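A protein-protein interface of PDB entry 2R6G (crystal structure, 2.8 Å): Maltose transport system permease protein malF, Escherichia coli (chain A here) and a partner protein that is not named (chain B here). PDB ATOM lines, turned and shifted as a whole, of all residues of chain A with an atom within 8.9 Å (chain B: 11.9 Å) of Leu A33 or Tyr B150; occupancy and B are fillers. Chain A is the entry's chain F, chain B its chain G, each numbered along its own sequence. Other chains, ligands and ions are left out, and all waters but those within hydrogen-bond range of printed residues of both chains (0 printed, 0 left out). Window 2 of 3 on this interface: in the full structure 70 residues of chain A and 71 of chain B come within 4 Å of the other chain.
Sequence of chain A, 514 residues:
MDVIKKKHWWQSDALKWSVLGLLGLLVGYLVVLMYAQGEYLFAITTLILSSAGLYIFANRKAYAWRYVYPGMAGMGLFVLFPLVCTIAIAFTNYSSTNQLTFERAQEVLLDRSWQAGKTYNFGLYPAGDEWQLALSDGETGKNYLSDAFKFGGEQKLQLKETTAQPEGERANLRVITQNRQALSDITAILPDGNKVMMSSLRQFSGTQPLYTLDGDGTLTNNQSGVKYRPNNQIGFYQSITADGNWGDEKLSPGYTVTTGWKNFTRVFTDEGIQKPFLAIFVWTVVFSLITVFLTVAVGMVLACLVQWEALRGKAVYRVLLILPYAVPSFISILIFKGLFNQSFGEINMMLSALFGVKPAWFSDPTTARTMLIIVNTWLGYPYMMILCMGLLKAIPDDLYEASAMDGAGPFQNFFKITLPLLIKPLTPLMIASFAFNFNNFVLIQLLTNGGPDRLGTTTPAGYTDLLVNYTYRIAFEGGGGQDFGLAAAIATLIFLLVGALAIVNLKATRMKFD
The side-chain carboxylate (OE2) of Glu A39 sits close to the side-chain carboxylate (OE1) of Glu B149 (2.9 Å).
The side-chain hydroxyl of Tyr B150 lies within hydrogen-bond range of the side-chain carboxylate of Glu A39, 3.4 Å away.
The side-chain carboxylate of Glu B149 sits close to the side-chain hydroxyl of Tyr B150, 3.4 Å away.
Among the printed residues, merely in contact across the chains: Glu A39 with Arg B146, Met A34 with Tyr B150, Phe A42 with Tyr B150, Leu A33 with Tyr B150, Phe A42 with Arg B146 and Phe A42 with Leu B143.
Printed residues of chain A within 4 Å of Tyr B150: Leu A33 (3.6 Å), Met A34 (3.4 Å), Glu A39 (3.4 Å) and Phe A42 (3.6 Å).
No residue of chain B comes within 4 Å of Gly A28.
No residue of chain B comes within 4 Å of Leu A30.
No residue of chain B comes within 4 Å of Val A31.
Met A34 touches one residue of chain B.
No residue of chain B comes within 4 Å of Ala A36.
No residue of chain B comes within 4 Å of Gly A38.
Printed residues of chain B within 4 Å of Glu A39: Arg B146, Glu B149 and Tyr B150.
No residue of chain A comes within 4 Å of Gly B148.
Glu B149 touches one residue of chain A.
No residue of chain A comes within 4 Å of Ile B151.
Of the printed residues of chain A, Arg B146 touches Glu A39 and Phe A42.
Printed residues of chain A within 4 Å of Leu B143: Phe A42 (3.9 Å).
Tyr A35 touches none of the printed residues of chain B.
Thr A46 touches none of the printed residues of chain B.
The nearest printed residue of chain A that does not touch Leu B143 is Glu A39 (7.6 Å).
Of the 18 printed residues of chain A, 4 touch a printed residue of chain B.
Printed residues of chain A that touch a printed residue of chain B: Leu A33, Met A34, Glu A39 and Phe A42.
Hydrophobic or aromatic side chains of chain A that line the printed part of chain B: Leu A33, Met A34 and Phe A42.
Of the 18 printed residues of chain B, 4 touch a printed residue of chain A.
Printed residues of chain B that touch a printed residue of chain A: Leu B143, Arg B146, Glu B149 and Tyr B150.
Hydrophobic or aromatic side chains of chain B within 4 Å of the printed part of chain A: Leu B143 and Tyr B150.
Among the printed residues, 8 pairs touch across the chains.
Among the printed residues, no Asp or Glu carboxylate lies within 4 Å of a Lys or Arg side-chain nitrogen of the other chain.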
ATOM      1  N   LEU A  26      13.214 -12.514  22.854  1.00  0.00           N
ATOM      2  CA  LEU A  26      11.939 -12.990  23.399  1.00  0.00           C
ATOM      3  C   LEU A  26      10.913 -13.264  22.300  1.00  0.00           C
ATOM      4  O   LEU A  26      10.209 -14.274  22.339  1.00  0.00           O
ATOM      5  CB  LEU A  26      11.376 -11.997  24.424  1.00  0.00           C
ATOM      6  CG  LEU A  26      12.156 -11.781  25.727  1.00  0.00           C
ATOM      7  CD1 LEU A  26      11.668 -10.527  26.437  1.00  0.00           C
ATOM      8  CD2 LEU A  26      12.072 -12.994  26.653  1.00  0.00           C
ATOM      9  N   VAL A  27      10.840 -12.360  21.325  1.00  0.00           N
ATOM     10  CA  VAL A  27      10.049 -12.579  20.118  1.00  0.00           C
ATOM     11  C   VAL A  27      10.780 -13.624  19.273  1.00  0.00           C
ATOM     12  O   VAL A  27      11.693 -13.307  18.506  1.00  0.00           O
ATOM     13  CB  VAL A  27       9.815 -11.263  19.331  1.00  0.00           C
ATOM     14  CG1 VAL A  27       9.027 -11.521  18.052  1.00  0.00           C
ATOM     15  CG2 VAL A  27       9.087 -10.244  20.202  1.00  0.00           C
ATOM     16  N   GLY A  28      10.374 -14.878  19.447  1.00  0.00           N
ATOM     17  CA  GLY A  28      11.081 -16.026  18.889  1.00  0.00           C
ATOM     18  C   GLY A  28      11.107 -17.124  19.932  1.00  0.00           C
ATOM     19  O   GLY A  28      10.655 -18.241  19.680  1.00  0.00           O
ATOM     20  N   TYR A  29      11.634 -16.794  21.111  1.00  0.00           N
ATOM     21  CA  TYR A  29      11.550 -17.665  22.283  1.00  0.00           C
ATOM     22  C   TYR A  29      10.098 -17.899  22.685  1.00  0.00           C
ATOM     23  O   TYR A  29       9.761 -18.946  23.236  1.00  0.00           O
ATOM     24  CB  TYR A  29      12.317 -17.064  23.463  1.00  0.00           C
ATOM     25  CG  TYR A  29      13.705 -17.628  23.658  1.00  0.00           C
ATOM     26  CD1 TYR A  29      14.809 -17.054  23.027  1.00  0.00           C
ATOM     27  CD2 TYR A  29      13.918 -18.733  24.484  1.00  0.00           C
ATOM     28  CE1 TYR A  29      16.090 -17.570  23.208  1.00  0.00           C
ATOM     29  CE2 TYR A  29      15.196 -19.257  24.672  1.00  0.00           C
ATOM     30  CZ  TYR A  29      16.276 -18.669  24.031  1.00  0.00           C
ATOM     31  OH  TYR A  29      17.540 -19.181  24.212  1.00  0.00           O
ATOM     32  N   LEU A  30       9.254 -16.905  22.411  1.00  0.00           N
ATOM     33  CA  LEU A  30       7.817 -16.998  22.654  1.00  0.00           C
ATOM     34  C   LEU A  30       7.067 -17.377  21.379  1.00  0.00           C
ATOM     35  O   LEU A  30       6.117 -18.156  21.430  1.00  0.00           O
ATOM     36  CB  LEU A  30       7.275 -15.676  23.216  1.00  0.00           C
ATOM     37  CG  LEU A  30       7.758 -15.209  24.595  1.00  0.00           C
ATOM     38  CD1 LEU A  30       7.613 -13.699  24.735  1.00  0.00           C
ATOM     39  CD2 LEU A  30       7.027 -15.928  25.727  1.00  0.00           C
ATOM     40  N   VAL A  31       7.509 -16.835  20.244  1.00  0.00           N
ATOM     41  CA  VAL A  31       6.838 -17.035  18.953  1.00  0.00           C
ATOM     42  C   VAL A  31       6.895 -18.490  18.474  1.00  0.00           C
ATOM     43  O   VAL A  31       5.856 -19.086  18.178  1.00  0.00           O
ATOM     44  CB  VAL A  31       7.391 -16.079  17.860  1.00  0.00           C
ATOM     45  CG1 VAL A  31       6.757 -16.369  16.502  1.00  0.00           C
ATOM     46  CG2 VAL A  31       7.148 -14.631  18.251  1.00  0.00           C
ATOM     47  N   VAL A  32       8.102 -19.050  18.404  1.00  0.00           N
ATOM     48  CA  VAL A  32       8.291 -20.445  17.989  1.00  0.00           C
ATOM     49  C   VAL A  32       7.689 -21.396  19.030  1.00  0.00           C
ATOM     50  O   VAL A  32       7.227 -22.490  18.694  1.00  0.00           O
ATOM     51  CB  VAL A  32       9.790 -20.780  17.726  1.00  0.00           C
ATOM     52  CG1 VAL A  32       9.954 -22.202  17.194  1.00  0.00           C
ATOM     53  CG2 VAL A  32      10.401 -19.786  16.743  1.00  0.00           C
ATOM     54  N   LEU A  33       7.685 -20.956  20.287  1.00  0.00           N
ATOM     55  CA  LEU A  33       7.053 -21.690  21.379  1.00  0.00           C
ATOM     56  C   LEU A  33       5.533 -21.741  21.200  1.00  0.00           C
ATOM     57  O   LEU A  33       4.897 -22.744  21.531  1.00  0.00           O
ATOM     58  CB  LEU A  33       7.424 -21.049  22.724  1.00  0.00           C
ATOM     59  CG  LEU A  33       7.401 -21.823  24.051  1.00  0.00           C
ATOM     60  CD1 LEU A  33       6.007 -21.857  24.668  1.00  0.00           C
ATOM     61  CD2 LEU A  33       7.982 -23.234  23.942  1.00  0.00           C
ATOM     62  N   MET A  34       4.963 -20.659  20.668  1.00  0.00           N
ATOM     63  CA  MET A  34       3.531 -20.589  20.359  1.00  0.00           C
ATOM     64  C   MET A  34       3.181 -21.380  19.102  1.00  0.00           C
ATOM     65  O   MET A  34       2.052 -21.860  18.959  1.00  0.00           O
ATOM     66  CB  MET A  34       3.079 -19.137  20.187  1.00  0.00           C
ATOM     67  CG  MET A  34       2.987 -18.352  21.479  1.00  0.00           C
ATOM     68  SD  MET A  34       2.805 -16.588  21.188  1.00  0.00           S
ATOM     69  CE  MET A  34       3.273 -15.931  22.788  1.00  0.00           C
ATOM     70  N   TYR A  35       4.149 -21.496  18.193  1.00  0.00           N
ATOM     71  CA  TYR A  35       3.991 -22.277  16.965  1.00  0.00           C
ATOM     72  C   TYR A  35       3.814 -23.758  17.295  1.00  0.00           C
ATOM     73  O   TYR A  35       3.000 -24.447  16.674  1.00  0.00           O
ATOM     74  CB  TYR A  35       5.187 -22.059  16.029  1.00  0.00           C
ATOM     75  CG  TYR A  35       5.167 -22.912  14.778  1.00  0.00           C
ATOM     76  CD1 TYR A  35       4.347 -22.584  13.697  1.00  0.00           C
ATOM     77  CD2 TYR A  35       5.975 -24.044  14.673  1.00  0.00           C
ATOM     78  CE1 TYR A  35       4.327 -23.366  12.548  1.00  0.00           C
ATOM     79  CE2 TYR A  35       5.963 -24.833  13.528  1.00  0.00           C
ATOM     80  CZ  TYR A  35       5.139 -24.487  12.471  1.00  0.00           C
ATOM     81  OH  TYR A  35       5.126 -25.266  11.338  1.00  0.00           O
ATOM     82  N   ALA A  36       4.580 -24.234  18.276  1.00  0.00           N
ATOM     83  CA  ALA A  36       4.421 -25.583  18.812  1.00  0.00           C
ATOM     84  C   ALA A  36       3.160 -25.661  19.677  1.00  0.00           C
ATOM     85  O   ALA A  36       2.489 -24.650  19.900  1.00  0.00           O
ATOM     86  CB  ALA A  36       5.654 -25.985  19.613  1.00  0.00           C
ATOM     87  N   GLN A  37       2.848 -26.866  20.154  1.00  0.00           N
ATOM     88  CA  GLN A  37       1.640 -27.150  20.952  1.00  0.00           C
ATOM     89  C   GLN A  37       0.319 -26.570  20.399  1.00  0.00           C
ATOM     90  O   GLN A  37      -0.640 -26.356  21.146  1.00  0.00           O
ATOM     91  CB  GLN A  37       1.847 -26.824  22.447  1.00  0.00           C
ATOM     92  CG  GLN A  37       2.069 -25.354  22.794  1.00  0.00           C
ATOM     93  CD  GLN A  37       2.504 -25.152  24.234  1.00  0.00           C
ATOM     94  OE1 GLN A  37       1.952 -25.754  25.155  1.00  0.00           O
ATOM     95  NE2 GLN A  37       3.498 -24.295  24.433  1.00  0.00           N
ATOM     96  N   GLY A  38       0.292 -26.328  19.088  1.00  0.00           N
ATOM     97  CA  GLY A  38      -0.930 -26.004  18.350  1.00  0.00           C
ATOM     98  C   GLY A  38      -1.687 -24.755  18.763  1.00  0.00           C
ATOM     99  O   GLY A  38      -2.865 -24.829  19.123  1.00  0.00           O
ATOM    100  N   GLU A  39      -1.010 -23.610  18.713  1.00  0.00           N
ATOM    101  CA  GLU A  39      -1.646 -22.315  18.950  1.00  0.00           C
ATOM    102  C   GLU A  39      -1.220 -21.338  17.856  1.00  0.00           C
ATOM    103  O   GLU A  39      -0.499 -20.369  18.112  1.00  0.00           O
ATOM    104  CB  GLU A  39      -1.305 -21.780  20.345  1.00  0.00           C
ATOM    105  CG  GLU A  39      -2.053 -22.479  21.476  1.00  0.00           C
ATOM    106  CD  GLU A  39      -1.775 -21.873  22.840  1.00  0.00           C
ATOM    107  OE1 GLU A  39      -1.861 -20.634  22.980  1.00  0.00           O
ATOM    108  OE2 GLU A  39      -1.483 -22.643  23.778  1.00  0.00           O
ATOM    109  N   TYR A  40      -1.687 -21.608  16.639  1.00  0.00           N
ATOM    110  CA  TYR A  40      -1.205 -20.929  15.433  1.00  0.00           C
ATOM    111  C   TYR A  40      -1.722 -19.503  15.253  1.00  0.00           C
ATOM    112  O   TYR A  40      -0.969 -18.624  14.826  1.00  0.00           O
ATOM    113  CB  TYR A  40      -1.502 -21.777  14.190  1.00  0.00           C
ATOM    114  CG  TYR A  40      -0.882 -23.157  14.248  1.00  0.00           C
ATOM    115  CD1 TYR A  40      -1.625 -24.259  14.669  1.00  0.00           C
ATOM    116  CD2 TYR A  40       0.455 -23.358  13.895  1.00  0.00           C
ATOM    117  CE1 TYR A  40      -1.058 -25.528  14.730  1.00  0.00           C
ATOM    118  CE2 TYR A  40       1.032 -24.622  13.953  1.00  0.00           C
ATOM    119  CZ  TYR A  40       0.270 -25.701  14.372  1.00  0.00           C
ATOM    120  OH  TYR A  40       0.832 -26.953  14.432  1.00  0.00           O
ATOM    121  N   PHE A  42      -2.490 -17.507  17.643  1.00  0.00           N
ATOM    122  CA  PHE A  42      -1.742 -16.741  18.636  1.00  0.00           C
ATOM    123  C   PHE A  42      -0.247 -16.653  18.316  1.00  0.00           C
ATOM    124  O   PHE A  42       0.459 -15.805  18.861  1.00  0.00           O
ATOM    125  CB  PHE A  42      -1.967 -17.311  20.039  1.00  0.00           C
ATOM    126  CG  PHE A  42      -1.724 -16.320  21.138  1.00  0.00           C
ATOM    127  CD1 PHE A  42      -0.629 -16.455  21.981  1.00  0.00           C
ATOM    128  CD2 PHE A  42      -2.587 -15.242  21.323  1.00  0.00           C
ATOM    129  CE1 PHE A  42      -0.396 -15.535  22.999  1.00  0.00           C
ATOM    130  CE2 PHE A  42      -2.363 -14.316  22.336  1.00  0.00           C
ATOM    131  CZ  PHE A  42      -1.264 -14.464  23.177  1.00  0.00           C
ATOM    132  N   ALA A  43       0.225 -17.528  17.432  1.00  0.00           N
ATOM    133  CA  ALA A  43       1.608 -17.492  16.962  1.00  0.00           C
ATOM    134  C   ALA A  43       1.774 -16.485  15.826  1.00  0.00           C
ATOM    135  O   ALA A  43       2.789 -15.789  15.750  1.00  0.00           O
ATOM    136  CB  ALA A  43       2.058 -18.877  16.520  1.00  0.00           C
ATOM    137  N   THR A  46       1.106 -12.655  17.206  1.00  0.00           N
ATOM    138  CA  THR A  46       2.207 -12.164  18.031  1.00  0.00           C
ATOM    139  C   THR A  46       3.446 -11.836  17.192  1.00  0.00           C
ATOM    140  O   THR A  46       4.319 -11.090  17.636  1.00  0.00           O
ATOM    141  CB  THR A  46       2.561 -13.156  19.168  1.00  0.00           C
ATOM    142  OG1 THR A  46       3.268 -12.467  20.206  1.00  0.00           O
ATOM    143  CG2 THR A  46       3.413 -14.310  18.652  1.00  0.00           C
ATOM    144  N   TYR B 141     -12.417 -13.966  26.376  1.00  0.00           N
ATOM    145  CA  TYR B 141     -12.080 -15.075  27.261  1.00  0.00           C
ATOM    146  C   TYR B 141     -11.033 -15.978  26.624  1.00  0.00           C
ATOM    147  O   TYR B 141     -10.142 -16.480  27.309  1.00  0.00           O
ATOM    148  CB  TYR B 141     -13.326 -15.885  27.633  1.00  0.00           C
ATOM    149  CG  TYR B 141     -13.096 -16.854  28.774  1.00  0.00           C
ATOM    150  CD1 TYR B 141     -13.245 -16.448  30.100  1.00  0.00           C
ATOM    151  CD2 TYR B 141     -12.722 -18.176  28.528  1.00  0.00           C
ATOM    152  CE1 TYR B 141     -13.031 -17.335  31.153  1.00  0.00           C
ATOM    153  CE2 TYR B 141     -12.504 -19.070  29.572  1.00  0.00           C
ATOM    154  CZ  TYR B 141     -12.660 -18.643  30.881  1.00  0.00           C
ATOM    155  OH  TYR B 141     -12.447 -19.525  31.917  1.00  0.00           O
ATOM    156  N   ALA B 142     -11.148 -16.175  25.313  1.00  0.00           N
ATOM    157  CA  ALA B 142     -10.184 -16.967  24.557  1.00  0.00           C
ATOM    158  C   ALA B 142      -8.808 -16.304  24.546  1.00  0.00           C
ATOM    159  O   ALA B 142      -7.796 -16.976  24.739  1.00  0.00           O
ATOM    160  CB  ALA B 142     -10.684 -17.198  23.139  1.00  0.00           C
ATOM    161  N   LEU B 143      -8.783 -14.986  24.343  1.00  0.00           N
ATOM    162  CA  LEU B 143      -7.536 -14.222  24.269  1.00  0.00           C
ATOM    163  C   LEU B 143      -6.742 -14.238  25.576  1.00  0.00           C
ATOM    164  O   LEU B 143      -5.544 -14.525  25.569  1.00  0.00           O
ATOM    165  CB  LEU B 143      -7.807 -12.779  23.823  1.00  0.00           C
ATOM    166  CG  LEU B 143      -6.647 -11.772  23.823  1.00  0.00           C
ATOM    167  CD1 LEU B 143      -5.534 -12.174  22.861  1.00  0.00           C
ATOM    168  CD2 LEU B 143      -7.154 -10.380  23.493  1.00  0.00           C
ATOM    169  N   PHE B 144      -7.411 -13.930  26.685  1.00  0.00           N
ATOM    170  CA  PHE B 144      -6.763 -13.880  27.999  1.00  0.00           C
ATOM    171  C   PHE B 144      -6.413 -15.262  28.541  1.00  0.00           C
ATOM    172  O   PHE B 144      -5.557 -15.394  29.420  1.00  0.00           O
ATOM    173  CB  PHE B 144      -7.621 -13.111  29.004  1.00  0.00           C
ATOM    174  CG  PHE B 144      -7.553 -11.621  28.838  1.00  0.00           C
ATOM    175  CD1 PHE B 144      -8.597 -10.925  28.240  1.00  0.00           C
ATOM    176  CD2 PHE B 144      -6.439 -10.910  29.274  1.00  0.00           C
ATOM    177  CE1 PHE B 144      -8.535  -9.542  28.082  1.00  0.00           C
ATOM    178  CE2 PHE B 144      -6.366  -9.528  29.120  1.00  0.00           C
ATOM    179  CZ  PHE B 144      -7.416  -8.844  28.526  1.00  0.00           C
ATOM    180  N   ASP B 145      -7.085 -16.284  28.013  1.00  0.00           N
ATOM    181  CA  ASP B 145      -6.729 -17.672  28.285  1.00  0.00           C
ATOM    182  C   ASP B 145      -5.411 -18.005  27.581  1.00  0.00           C
ATOM    183  O   ASP B 145      -4.566 -18.710  28.134  1.00  0.00           O
ATOM    184  CB  ASP B 145      -7.844 -18.612  27.818  1.00  0.00           C
ATOM    185  CG  ASP B 145      -7.790 -19.973  28.493  1.00  0.00           C
ATOM    186  OD1 ASP B 145      -7.344 -20.058  29.659  1.00  0.00           O
ATOM    187  OD2 ASP B 145      -8.211 -20.963  27.857  1.00  0.00           O
ATOM    188  N   ARG B 146      -5.246 -17.483  26.366  1.00  0.00           N
ATOM    189  CA  ARG B 146      -3.998 -17.619  25.619  1.00  0.00           C
ATOM    190  C   ARG B 146      -2.890 -16.735  26.192  1.00  0.00           C
ATOM    191  O   ARG B 146      -1.722 -17.116  26.184  1.00  0.00           O
ATOM    192  CB  ARG B 146      -4.210 -17.304  24.131  1.00  0.00           C
ATOM    193  CG  ARG B 146      -4.500 -18.522  23.244  1.00  0.00           C
ATOM    194  CD  ARG B 146      -5.967 -18.933  23.277  1.00  0.00           C
ATOM    195  NE  ARG B 146      -6.282 -19.972  22.295  1.00  0.00           N
ATOM    196  CZ  ARG B 146      -7.488 -20.511  22.122  1.00  0.00           C
ATOM    197  NH1 ARG B 146      -8.519 -20.119  22.864  1.00  0.00           N
ATOM    198  NH2 ARG B 146      -7.666 -21.449  21.203  1.00  0.00           N
ATOM    199  N   LEU B 147      -3.262 -15.556  26.683  1.00  0.00           N
ATOM    200  CA  LEU B 147      -2.300 -14.633  27.283  1.00  0.00           C
ATOM    201  C   LEU B 147      -1.707 -15.175  28.580  1.00  0.00           C
ATOM    202  O   LEU B 147      -0.489 -15.169  28.758  1.00  0.00           O
ATOM    203  CB  LEU B 147      -2.941 -13.264  27.530  1.00  0.00           C
ATOM    204  CG  LEU B 147      -2.694 -12.169  26.493  1.00  0.00           C
ATOM    205  CD1 LEU B 147      -3.784 -11.111  26.561  1.00  0.00           C
ATOM    206  CD2 LEU B 147      -1.317 -11.541  26.687  1.00  0.00           C
ATOM    207  N   GLY B 148      -2.580 -15.655  29.465  1.00  0.00           N
ATOM    208  CA  GLY B 148      -2.199 -16.089  30.809  1.00  0.00           C
ATOM    209  C   GLY B 148      -1.101 -17.131  30.886  1.00  0.00           C
ATOM    210  O   GLY B 148      -0.274 -17.100  31.799  1.00  0.00           O
ATOM    211  N   GLU B 149      -1.096 -18.051  29.924  1.00  0.00           N
ATOM    212  CA  GLU B 149      -0.115 -19.138  29.883  1.00  0.00           C
ATOM    213  C   GLU B 149       1.283 -18.680  29.457  1.00  0.00           C
ATOM    214  O   GLU B 149       2.274 -19.342  29.770  1.00  0.00           O
ATOM    215  CB  GLU B 149      -0.603 -20.278  28.983  1.00  0.00           C
ATOM    216  CG  GLU B 149      -1.102 -19.829  27.617  1.00  0.00           C
ATOM    217  CD  GLU B 149      -1.305 -20.979  26.652  1.00  0.00           C
ATOM    218  OE1 GLU B 149      -0.304 -21.626  26.275  1.00  0.00           O
ATOM    219  OE2 GLU B 149      -2.468 -21.225  26.261  1.00  0.00           O
ATOM    220  N   TYR B 150       1.359 -17.558  28.745  1.00  0.00           N
ATOM    221  CA  TYR B 150       2.647 -17.016  28.311  1.00  0.00           C
ATOM    222  C   TYR B 150       3.095 -15.856  29.192  1.00  0.00           C
ATOM    223  O   TYR B 150       4.201 -15.874  29.737  1.00  0.00           O
ATOM    224  CB  TYR B 150       2.607 -16.614  26.834  1.00  0.00           C
ATOM    225  CG  TYR B 150       2.306 -17.776  25.917  1.00  0.00           C
ATOM    226  CD1 TYR B 150       1.067 -17.890  25.296  1.00  0.00           C
ATOM    227  CD2 TYR B 150       3.253 -18.775  25.688  1.00  0.00           C
ATOM    228  CE1 TYR B 150       0.777 -18.964  24.458  1.00  0.00           C
ATOM    229  CE2 TYR B 150       2.975 -19.851  24.854  1.00  0.00           C
ATOM    230  CZ  TYR B 150       1.735 -19.941  24.244  1.00  0.00           C
ATOM    231  OH  TYR B 150       1.452 -21.003  23.413  1.00  0.00           O
ATOM    232  N   ILE B 151       2.236 -14.851  29.328  1.00  0.00           N
ATOM    233  CA  ILE B 151       2.465 -13.776  30.284  1.00  0.00           C
ATOM    234  C   ILE B 151       1.359 -13.821  31.337  1.00  0.00           C
ATOM    235  O   ILE B 151       0.217 -13.441  31.057  1.00  0.00           O
ATOM    236  CB  ILE B 151       2.537 -12.367  29.611  1.00  0.00           C
ATOM    237  CG1 ILE B 151       3.454 -12.373  28.373  1.00  0.00           C
ATOM    238  CG2 ILE B 151       2.968 -11.296  30.625  1.00  0.00           C
ATOM    239  CD1 ILE B 151       4.929 -12.727  28.636  1.00  0.00           C
ATOM    240  N   PRO B 152       1.687 -14.321  32.545  1.00  0.00           N
ATOM    241  CA  PRO B 152       0.756 -14.294  33.674  1.00  0.00           C
ATOM    242  C   PRO B 152       0.512 -12.865  34.170  1.00  0.00           C
ATOM    243  O   PRO B 152       0.905 -11.903  33.501  1.00  0.00           O
ATOM    244  CB  PRO B 152       1.475 -15.130  34.747  1.00  0.00           C
ATOM    245  CG  PRO B 152       2.548 -15.879  34.017  1.00  0.00           C
ATOM    246  CD  PRO B 152       2.957 -14.974  32.907  1.00  0.00           C
ATOM    247  N   PHE B 153      -0.129 -12.741  35.330  1.00  0.00           N
ATOM    248  CA  PHE B 153      -0.558 -11.453  35.913  1.00  0.00           C
ATOM    249  C   PHE B 153      -1.352 -10.497  35.001  1.00  0.00           C
ATOM    250  O   PHE B 153      -1.920  -9.512  35.478  1.00  0.00           O
ATOM    251  CB  PHE B 153       0.563 -10.736  36.705  1.00  0.00           C
ATOM    252  CG  PHE B 153       1.670 -10.162  35.856  1.00  0.00           C
ATOM    253  CD1 PHE B 153       2.888 -10.835  35.731  1.00  0.00           C
ATOM    254  CD2 PHE B 153       1.514  -8.933  35.215  1.00  0.00           C
ATOM    255  CE1 PHE B 153       3.923 -10.308  34.958  1.00  0.00           C
ATOM    256  CE2 PHE B 153       2.543  -8.395  34.439  1.00  0.00           C
ATOM    257  CZ  PHE B 153       3.751  -9.084  34.311  1.00  0.00           C
ATOM    258  N   ILE B 154      -1.378 -10.793  33.701  1.00  0.00           N
ATOM    259  CA  ILE B 154      -2.255 -10.093  32.756  1.00  0.00           C
ATOM    260  C   ILE B 154      -3.192 -11.063  32.024  1.00  0.00           C
ATOM    261  O   ILE B 154      -3.770 -10.721  30.989  1.00  0.00           O
ATOM    262  CB  ILE B 154      -1.482  -9.195  31.735  1.00  0.00           C
ATOM    263  CG1 ILE B 154      -0.464 -10.009  30.930  1.00  0.00           C
ATOM    264  CG2 ILE B 154      -0.832  -7.999  32.442  1.00  0.00           C
ATOM    265  CD1 ILE B 154      -0.066  -9.369  29.609  1.00  0.00           C
ATOM    266  N   GLY B 155      -3.335 -12.268  32.573  1.00  0.00           N
ATOM    267  CA  GLY B 155      -4.232 -13.280  32.014  1.00  0.00           C
ATOM    268  C   GLY B 155      -5.575 -13.319  32.717  1.00  0.00           C
ATOM    269  O   GLY B 155      -6.110 -12.280  33.108  1.00  0.00           O
ATOM    270  N   LEU B 156      -6.122 -14.522  32.872  1.00  0.00           N
ATOM    271  CA  LEU B 156      -7.388 -14.712  33.578  1.00  0.00           C
ATOM    272  C   LEU B 156      -7.213 -14.573  35.089  1.00  0.00           C
ATOM    273  O   LEU B 156      -6.122 -14.794  35.616  1.00  0.00           O
ATOM    274  CB  LEU B 156      -7.995 -16.077  33.238  1.00  0.00           C
ATOM    275  CG  LEU B 156      -8.643 -16.261  31.861  1.00  0.00           C
ATOM    276  CD1 LEU B 156      -8.950 -17.729  31.608  1.00  0.00           C
ATOM    277  CD2 LEU B 156      -9.908 -15.419  31.726  1.00  0.00           C
ATOM    278  N   THR B 158      -7.015 -11.991  37.171  1.00  0.00           N
ATOM    279  CA  THR B 158      -6.018 -11.021  37.634  1.00  0.00           C
ATOM    280  C   THR B 158      -6.367  -9.605  37.182  1.00  0.00           C
ATOM    281  O   THR B 158      -6.940  -9.415  36.107  1.00  0.00           O
ATOM    282  CB  THR B 158      -4.574 -11.404  37.194  1.00  0.00           C
ATOM    283  OG1 THR B 158      -3.687 -10.300  37.419  1.00  0.00           O
ATOM    284  CG2 THR B 158      -4.528 -11.788  35.728  1.00  0.00           C
ATOM    285  N   PHE B 164      -5.966  -4.225  31.281  1.00  0.00           N
ATOM    286  CA  PHE B 164      -5.439  -4.316  29.925  1.00  0.00           C
ATOM    287  C   PHE B 164      -6.577  -4.395  28.914  1.00  0.00           C
ATOM    288  O   PHE B 164      -6.455  -3.900  27.799  1.00  0.00           O
ATOM    289  CB  PHE B 164      -4.530  -5.539  29.790  1.00  0.00           C
ATOM    290  CG  PHE B 164      -3.193  -5.242  29.166  1.00  0.00           C
ATOM    291  CD1 PHE B 164      -2.162  -4.689  29.928  1.00  0.00           C
ATOM    292  CD2 PHE B 164      -2.957  -5.529  27.825  1.00  0.00           C
ATOM    293  CE1 PHE B 164      -0.912  -4.416  29.358  1.00  0.00           C
ATOM    294  CE2 PHE B 164      -1.714  -5.262  27.243  1.00  0.00           C
ATOM    295  CZ  PHE B 164      -0.689  -4.704  28.014  1.00  0.00           C
